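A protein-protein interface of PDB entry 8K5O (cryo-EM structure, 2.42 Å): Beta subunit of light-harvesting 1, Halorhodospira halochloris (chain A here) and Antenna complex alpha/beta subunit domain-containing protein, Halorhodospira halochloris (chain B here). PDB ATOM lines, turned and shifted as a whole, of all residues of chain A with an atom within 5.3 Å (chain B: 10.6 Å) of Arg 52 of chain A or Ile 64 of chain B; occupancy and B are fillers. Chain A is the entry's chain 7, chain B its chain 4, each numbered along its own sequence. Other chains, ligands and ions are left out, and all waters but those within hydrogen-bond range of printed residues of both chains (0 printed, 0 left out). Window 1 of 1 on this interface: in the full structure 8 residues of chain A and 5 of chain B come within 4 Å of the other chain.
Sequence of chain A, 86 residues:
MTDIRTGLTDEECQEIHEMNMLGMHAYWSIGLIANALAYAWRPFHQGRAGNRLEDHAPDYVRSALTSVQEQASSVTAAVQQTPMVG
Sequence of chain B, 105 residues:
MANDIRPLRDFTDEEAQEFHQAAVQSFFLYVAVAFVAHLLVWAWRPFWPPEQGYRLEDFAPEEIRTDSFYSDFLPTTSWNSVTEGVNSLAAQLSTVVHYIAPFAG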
ATOM      1  N   GLY A  50      27.141  -1.893   5.614  1.00  0.00           N
ATOM      2  CA  GLY A  50      26.620  -3.240   5.628  1.00  0.00           C
ATOM      3  C   GLY A  50      27.718  -4.252   5.388  1.00  0.00           C
ATOM      4  O   GLY A  50      28.894  -3.928   5.230  1.00  0.00           O
ATOM      5  N   ASN A  51      27.319  -5.519   5.370  1.00  0.00           N
ATOM      6  CA  ASN A  51      28.238  -6.581   4.992  1.00  0.00           C
ATOM      7  C   ASN A  51      27.554  -7.589   4.084  1.00  0.00           C
ATOM      8  O   ASN A  51      27.890  -8.777   4.103  1.00  0.00           O
ATOM      9  CB  ASN A  51      28.839  -7.277   6.218  1.00  0.00           C
ATOM     10  CG  ASN A  51      27.803  -7.657   7.250  1.00  0.00           C
ATOM     11  OD1 ASN A  51      26.682  -8.025   6.918  1.00  0.00           O
ATOM     12  ND2 ASN A  51      28.181  -7.576   8.515  1.00  0.00           N
ATOM     13  N   ARG A  52      26.588  -7.134   3.293  1.00  0.00           N
ATOM     14  CA  ARG A  52      25.998  -7.981   2.271  1.00  0.00           C
ATOM     15  C   ARG A  52      27.006  -8.215   1.155  1.00  0.00           C
ATOM     16  O   ARG A  52      27.693  -7.290   0.715  1.00  0.00           O
ATOM     17  CB  ARG A  52      24.728  -7.340   1.714  1.00  0.00           C
ATOM     18  CG  ARG A  52      23.511  -7.549   2.586  1.00  0.00           C
ATOM     19  CD  ARG A  52      22.276  -6.869   2.037  1.00  0.00           C
ATOM     20  NE  ARG A  52      22.595  -5.670   1.277  1.00  0.00           N
ATOM     21  CZ  ARG A  52      21.695  -4.930   0.643  1.00  0.00           C
ATOM     22  NH1 ARG A  52      20.410  -5.234   0.668  1.00  0.00           N
ATOM     23  NH2 ARG A  52      22.098  -3.861  -0.035  1.00  0.00           N
ATOM     24  N   LEU A  53      27.098  -9.466   0.704  1.00  0.00           N
ATOM     25  CA  LEU A  53      28.049  -9.800  -0.349  1.00  0.00           C
ATOM     26  C   LEU A  53      27.733  -9.044  -1.629  1.00  0.00           C
ATOM     27  O   LEU A  53      28.642  -8.582  -2.326  1.00  0.00           O
ATOM     28  CB  LEU A  53      28.042 -11.305  -0.608  1.00  0.00           C
ATOM     29  CG  LEU A  53      29.013 -12.161   0.199  1.00  0.00           C
ATOM     30  CD1 LEU A  53      28.966 -13.593  -0.302  1.00  0.00           C
ATOM     31  CD2 LEU A  53      30.422 -11.605   0.122  1.00  0.00           C
ATOM     32  N   GLU A  54      26.447  -8.895  -1.943  1.00  0.00           N
ATOM     33  CA  GLU A  54      26.043  -8.253  -3.188  1.00  0.00           C
ATOM     34  C   GLU A  54      26.550  -6.821  -3.291  1.00  0.00           C
ATOM     35  O   GLU A  54      26.784  -6.327  -4.400  1.00  0.00           O
ATOM     36  CB  GLU A  54      24.523  -8.296  -3.311  1.00  0.00           C
ATOM     37  CG  GLU A  54      23.800  -7.556  -2.204  1.00  0.00           C
ATOM     38  CD  GLU A  54      22.302  -7.692  -2.306  1.00  0.00           C
ATOM     39  OE1 GLU A  54      21.828  -8.378  -3.233  1.00  0.00           O
ATOM     40  OE2 GLU A  54      21.593  -7.117  -1.461  1.00  0.00           O
ATOM     41  N   ASP A  55      26.729  -6.139  -2.162  1.00  0.00           N
ATOM     42  CA  ASP A  55      27.198  -4.761  -2.182  1.00  0.00           C
ATOM     43  C   ASP A  55      28.711  -4.639  -2.261  1.00  0.00           C
ATOM     44  O   ASP A  55      29.210  -3.540  -2.515  1.00  0.00           O
ATOM     45  CB  ASP A  55      26.703  -4.016  -0.943  1.00  0.00           C
ATOM     46  CG  ASP A  55      25.197  -3.993  -0.841  1.00  0.00           C
ATOM     47  OD1 ASP A  55      24.530  -3.781  -1.874  1.00  0.00           O
ATOM     48  OD2 ASP A  55      24.677  -4.187   0.274  1.00  0.00           O
ATOM     49  N   HIS A  56      29.453  -5.723  -2.051  1.00  0.00           N
ATOM     50  CA  HIS A  56      30.903  -5.611  -1.971  1.00  0.00           C
ATOM     51  C   HIS A  56      31.615  -6.597  -2.886  1.00  0.00           C
ATOM     52  O   HIS A  56      32.709  -6.309  -3.380  1.00  0.00           O
ATOM     53  CB  HIS A  56      31.352  -5.797  -0.521  1.00  0.00           C
ATOM     54  CG  HIS A  56      30.683  -4.860   0.433  1.00  0.00           C
ATOM     55  ND1 HIS A  56      29.570  -5.210   1.165  1.00  0.00           N
ATOM     56  CD2 HIS A  56      30.957  -3.575   0.758  1.00  0.00           C
ATOM     57  CE1 HIS A  56      29.194  -4.184   1.908  1.00  0.00           C
ATOM     58  NE2 HIS A  56      30.020  -3.180   1.681  1.00  0.00           N
ATOM     59  N   ALA A  57      31.009  -7.756  -3.120  1.00  0.00           N
ATOM     60  CA  ALA A  57      31.616  -8.752  -3.985  1.00  0.00           C
ATOM     61  C   ALA A  57      31.558  -8.296  -5.445  1.00  0.00           C
ATOM     62  O   ALA A  57      30.700  -7.494  -5.819  1.00  0.00           O
ATOM     63  CB  ALA A  57      30.911 -10.094  -3.818  1.00  0.00           C
ATOM     64  N   LEU A  65      21.358 -13.944  -0.457  1.00  0.00           N
ATOM     65  CA  LEU A  65      20.426 -12.884  -0.107  1.00  0.00           C
ATOM     66  C   LEU A  65      19.711 -12.340  -1.337  1.00  0.00           C
ATOM     67  O   LEU A  65      18.586 -11.851  -1.246  1.00  0.00           O
ATOM     68  CB  LEU A  65      21.162 -11.757   0.613  1.00  0.00           C
ATOM     69  CG  LEU A  65      21.784 -12.158   1.949  1.00  0.00           C
ATOM     70  CD1 LEU A  65      22.616 -11.026   2.514  1.00  0.00           C
ATOM     71  CD2 LEU A  65      20.711 -12.586   2.932  1.00  0.00           C
ATOM     72  N   ARG B  45      23.078   1.625  15.077  1.00  0.00           N
ATOM     73  CA  ARG B  45      22.072   2.163  14.176  1.00  0.00           C
ATOM     74  C   ARG B  45      20.909   2.718  14.984  1.00  0.00           C
ATOM     75  O   ARG B  45      20.176   1.950  15.619  1.00  0.00           O
ATOM     76  CB  ARG B  45      21.589   1.092  13.200  1.00  0.00           C
ATOM     77  CG  ARG B  45      22.619   0.738  12.164  1.00  0.00           C
ATOM     78  CD  ARG B  45      22.104  -0.222  11.152  1.00  0.00           C
ATOM     79  NE  ARG B  45      23.117  -0.470  10.140  1.00  0.00           N
ATOM     80  CZ  ARG B  45      22.923  -1.195   9.052  1.00  0.00           C
ATOM     81  NH1 ARG B  45      21.746  -1.729   8.780  1.00  0.00           N
ATOM     82  NH2 ARG B  45      23.927  -1.362   8.199  1.00  0.00           N
ATOM     83  N   ARG B  55      15.006   4.949   5.593  1.00  0.00           N
ATOM     84  CA  ARG B  55      14.837   3.897   4.605  1.00  0.00           C
ATOM     85  C   ARG B  55      16.032   3.906   3.663  1.00  0.00           C
ATOM     86  O   ARG B  55      16.405   4.953   3.130  1.00  0.00           O
ATOM     87  CB  ARG B  55      13.542   4.107   3.835  1.00  0.00           C
ATOM     88  CG  ARG B  55      12.321   3.628   4.560  1.00  0.00           C
ATOM     89  CD  ARG B  55      11.146   3.549   3.622  1.00  0.00           C
ATOM     90  NE  ARG B  55      11.047   4.749   2.803  1.00  0.00           N
ATOM     91  CZ  ARG B  55       9.992   5.068   2.070  1.00  0.00           C
ATOM     92  NH1 ARG B  55       8.910   4.310   2.052  1.00  0.00           N
ATOM     93  NH2 ARG B  55      10.019   6.181   1.344  1.00  0.00           N
ATOM     94  N   LEU B  56      16.638   2.734   3.464  1.00  0.00           N
ATOM     95  CA  LEU B  56      17.829   2.656   2.627  1.00  0.00           C
ATOM     96  C   LEU B  56      17.536   3.065   1.189  1.00  0.00           C
ATOM     97  O   LEU B  56      18.406   3.625   0.515  1.00  0.00           O
ATOM     98  CB  LEU B  56      18.407   1.242   2.678  1.00  0.00           C
ATOM     99  CG  LEU B  56      19.814   1.060   2.109  1.00  0.00           C
ATOM    100  CD1 LEU B  56      20.837   1.870   2.882  1.00  0.00           C
ATOM    101  CD2 LEU B  56      20.187  -0.406   2.089  1.00  0.00           C
ATOM    102  N   GLU B  57      16.320   2.804   0.711  1.00  0.00           N
ATOM    103  CA  GLU B  57      15.946   3.192  -0.644  1.00  0.00           C
ATOM    104  C   GLU B  57      15.957   4.702  -0.830  1.00  0.00           C
ATOM    105  O   GLU B  57      16.099   5.185  -1.958  1.00  0.00           O
ATOM    106  CB  GLU B  57      14.570   2.621  -0.971  1.00  0.00           C
ATOM    107  CG  GLU B  57      13.464   3.141  -0.076  1.00  0.00           C
ATOM    108  CD  GLU B  57      12.134   2.493  -0.373  1.00  0.00           C
ATOM    109  OE1 GLU B  57      12.081   1.630  -1.271  1.00  0.00           O
ATOM    110  OE2 GLU B  57      11.138   2.847   0.287  1.00  0.00           O
ATOM    111  N   ASP B  58      15.809   5.464   0.252  1.00  0.00           N
ATOM    112  CA  ASP B  58      15.775   6.915   0.149  1.00  0.00           C
ATOM    113  C   ASP B  58      17.158   7.546   0.074  1.00  0.00           C
ATOM    114  O   ASP B  58      17.257   8.741  -0.217  1.00  0.00           O
ATOM    115  CB  ASP B  58      15.010   7.505   1.333  1.00  0.00           C
ATOM    116  CG  ASP B  58      13.518   7.280   1.230  1.00  0.00           C
ATOM    117  OD1 ASP B  58      12.943   7.584   0.165  1.00  0.00           O
ATOM    118  OD2 ASP B  58      12.918   6.805   2.213  1.00  0.00           O
ATOM    119  N   PHE B  59      18.220   6.782   0.319  1.00  0.00           N
ATOM    120  CA  PHE B  59      19.555   7.360   0.385  1.00  0.00           C
ATOM    121  C   PHE B  59      20.536   6.611  -0.505  1.00  0.00           C
ATOM    122  O   PHE B  59      21.472   7.208  -1.043  1.00  0.00           O
ATOM    123  CB  PHE B  59      20.053   7.366   1.828  1.00  0.00           C
ATOM    124  CG  PHE B  59      19.208   8.189   2.754  1.00  0.00           C
ATOM    125  CD1 PHE B  59      18.090   7.645   3.360  1.00  0.00           C
ATOM    126  CD2 PHE B  59      19.526   9.506   3.011  1.00  0.00           C
ATOM    127  CE1 PHE B  59      17.312   8.396   4.206  1.00  0.00           C
ATOM    128  CE2 PHE B  59      18.749  10.261   3.856  1.00  0.00           C
ATOM    129  CZ  PHE B  59      17.641   9.706   4.452  1.00  0.00           C
ATOM    130  N   ALA B  60      20.332   5.315  -0.662  1.00  0.00           N
ATOM    131  CA  ALA B  60      21.262   4.515  -1.438  1.00  0.00           C
ATOM    132  C   ALA B  60      20.966   4.639  -2.929  1.00  0.00           C
ATOM    133  O   ALA B  60      19.823   4.877  -3.327  1.00  0.00           O
ATOM    134  CB  ALA B  60      21.184   3.053  -1.017  1.00  0.00           C
ATOM    135  N   PRO B  61      21.982   4.488  -3.774  1.00  0.00           N
ATOM    136  CA  PRO B  61      21.742   4.440  -5.219  1.00  0.00           C
ATOM    137  C   PRO B  61      20.996   3.170  -5.598  1.00  0.00           C
ATOM    138  O   PRO B  61      20.908   2.209  -4.833  1.00  0.00           O
ATOM    139  CB  PRO B  61      23.149   4.468  -5.822  1.00  0.00           C
ATOM    140  CG  PRO B  61      24.032   4.978  -4.726  1.00  0.00           C
ATOM    141  CD  PRO B  61      23.417   4.507  -3.455  1.00  0.00           C
ATOM    142  N   GLU B  62      20.446   3.179  -6.812  1.00  0.00           N
ATOM    143  CA  GLU B  62      19.625   2.061  -7.262  1.00  0.00           C
ATOM    144  C   GLU B  62      20.422   0.777  -7.433  1.00  0.00           C
ATOM    145  O   GLU B  62      19.825  -0.302  -7.495  1.00  0.00           O
ATOM    146  CB  GLU B  62      18.919   2.419  -8.571  1.00  0.00           C
ATOM    147  CG  GLU B  62      17.782   3.417  -8.406  1.00  0.00           C
ATOM    148  CD  GLU B  62      16.508   2.781  -7.866  1.00  0.00           C
ATOM    149  OE1 GLU B  62      16.512   1.562  -7.594  1.00  0.00           O
ATOM    150  OE2 GLU B  62      15.500   3.504  -7.712  1.00  0.00           O
ATOM    151  N   GLU B  63      21.753   0.860  -7.506  1.00  0.00           N
ATOM    152  CA  GLU B  63      22.570  -0.344  -7.543  1.00  0.00           C
ATOM    153  C   GLU B  63      22.581  -1.084  -6.214  1.00  0.00           C
ATOM    154  O   GLU B  63      23.022  -2.237  -6.169  1.00  0.00           O
ATOM    155  CB  GLU B  63      24.002   0.002  -7.954  1.00  0.00           C
ATOM    156  CG  GLU B  63      24.142   0.439  -9.404  1.00  0.00           C
ATOM    157  CD  GLU B  63      23.825   1.907  -9.609  1.00  0.00           C
ATOM    158  OE1 GLU B  63      23.559   2.607  -8.609  1.00  0.00           O
ATOM    159  OE2 GLU B  63      23.839   2.361 -10.772  1.00  0.00           O
ATOM    160  N   ILE B  64      22.110  -0.456  -5.142  1.00  0.00           N
ATOM    161  CA  ILE B  64      22.025  -1.084  -3.831  1.00  0.00           C
ATOM    162  C   ILE B  64      20.627  -1.662  -3.685  1.00  0.00           C
ATOM    163  O   ILE B  64      19.631  -0.940  -3.809  1.00  0.00           O
ATOM    164  CB  ILE B  64      22.332  -0.081  -2.709  1.00  0.00           C
ATOM    165  CG1 ILE B  64      23.726   0.513  -2.899  1.00  0.00           C
ATOM    166  CG2 ILE B  64      22.214  -0.748  -1.351  1.00  0.00           C
ATOM    167  CD1 ILE B  64      24.838  -0.508  -2.850  1.00  0.00           C
ATOM    168  N   ARG B  65      20.549  -2.965  -3.431  1.00  0.00           N
ATOM    169  CA  ARG B  65      19.265  -3.642  -3.298  1.00  0.00           C
ATOM    170  C   ARG B  65      18.655  -3.286  -1.951  1.00  0.00           C
ATOM    171  O   ARG B  65      19.201  -3.630  -0.900  1.00  0.00           O
ATOM    172  CB  ARG B  65      19.434  -5.152  -3.433  1.00  0.00           C
ATOM    173  CG  ARG B  65      18.130  -5.913  -3.328  1.00  0.00           C
ATOM    174  CD  ARG B  65      18.354  -7.405  -3.434  1.00  0.00           C
ATOM    175  NE  ARG B  65      19.198  -7.904  -2.356  1.00  0.00           N
ATOM    176  CZ  ARG B  65      18.767  -8.193  -1.136  1.00  0.00           C
ATOM    177  NH1 ARG B  65      17.498  -8.037  -0.798  1.00  0.00           N
ATOM    178  NH2 ARG B  65      19.631  -8.650  -0.235  1.00  0.00           N
ATOM    179  N   THR B  66      17.520  -2.599  -1.984  1.00  0.00           N
ATOM    180  CA  THR B  66      16.767  -2.251  -0.790  1.00  0.00           C
ATOM    181  C   THR B  66      15.436  -2.981  -0.829  1.00  0.00           C
ATOM    182  O   THR B  66      14.719  -2.919  -1.832  1.00  0.00           O
ATOM    183  CB  THR B  66      16.541  -0.741  -0.697  1.00  0.00           C
ATOM    184  OG1 THR B  66      15.579  -0.341  -1.679  1.00  0.00           O
ATOM    185  CG2 THR B  66      17.839   0.012  -0.929  1.00  0.00           C
ATOM    186  N   ASP B  67      15.114  -3.679   0.252  1.00  0.00           N
ATOM    187  CA  ASP B  67      13.875  -4.432   0.359  1.00  0.00           C
ATOM    188  C   ASP B  67      12.996  -3.773   1.412  1.00  0.00           C
ATOM    189  O   ASP B  67      13.439  -3.551   2.542  1.00  0.00           O
ATOM    190  CB  ASP B  67      14.155  -5.891   0.727  1.00  0.00           C
ATOM    191  CG  ASP B  67      12.952  -6.788   0.520  1.00  0.00           C
ATOM    192  OD1 ASP B  67      11.894  -6.285   0.090  1.00  0.00           O
ATOM    193  OD2 ASP B  67      13.067  -8.003   0.791  1.00  0.00           O
ATOM    194  N   SER B  68      11.763  -3.455   1.036  1.00  0.00           N
ATOM    195  CA  SER B  68      10.849  -2.799   1.958  1.00  0.00           C
ATOM    196  C   SER B  68      10.483  -3.726   3.109  1.00  0.00           C
ATOM    197  O   SER B  68      10.484  -4.953   2.974  1.00  0.00           O
ATOM    198  CB  SER B  68       9.588  -2.351   1.227  1.00  0.00           C
ATOM    199  OG  SER B  68       8.855  -3.468   0.758  1.00  0.00           O
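NE of Arg 65 of chain B lies within salt-bridge range of OE2 of Glu 54 of chain A, at 2.7 Å.
The backbone carbonyl oxygen of Arg 65 of chain B is in hydrogen-bond range of the guanidinium group of Arg 52 of chain A (2.5 Å).
Of the 9 printed residues of chain A, 4 touch a printed residue of chain B.
Hydrophobic or aromatic side chains of chain A within 4 Å of the printed part of chain B: Leu 65.
Of the 15 printed residues of chain B, 2 touch a printed residue of chain A.
Hydrophobic or aromatic side chains of chain B within 4 Å of the printed part of chain A: Ile 64.
Among the printed residues, 5 pairs touch across the chains.
Among the printed residues, Asp or Glu carboxylates within 4 Å of a Lys or Arg side-chain nitrogen of the other chain: Glu 54 of chain A with Arg 65 of chain B (2.7 Å).
Of the printed residues of chain B, Arg 52 of chain A touches Ile 64 and Arg 65.
Ile 64 of chain B touches two residues of chain A.
No residue of chain B comes within 4 Å of Gly 50 of chain A.
Asn 51 of chain A touches none of the printed residues of chain B.
Printed residues of chain B within 4 Å of Glu 54 of chain A: Arg 65 (2.7 Å).
Printed residues of chain A within 4 Å of Arg 65 of chain B: Arg 52, Glu 54 and Leu 65.
Of the printed residues of chain B, Leu 65 of chain A touches Arg 65.
Asp 67 of chain B touches none of the printed residues of chain A.
The nearest residue of chain B that does not touch Arg 52 of chain A is Leu 56 of chain B (4.5 Å).
O of Arg 52 of chain A lies within hydrogen-bond range of ND1 of His 56 of chain A (2.8 Å).
The guanidinium group (NH1) of Arg 52 of chain A lies within salt-bridge range of the side-chain carboxylate (OE2) of Glu 54 of chain A, 3.1 Å away.
The guanidinium group (NH2) of Arg 52 of chain A is in salt-bridge range of the side-chain carboxylate (OD2) of Asp 55 of chain A, 2.6 Å away.
Among the printed residues, pairs that only touch across the chains: Arg 52 of chain A with Ile 64 of chain B (3.4 Å), Asp 55 of chain A with Ile 64 of chain B (3.4 Å) and Leu 65 of chain A with Arg 65 of chain B (3.5 Å).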
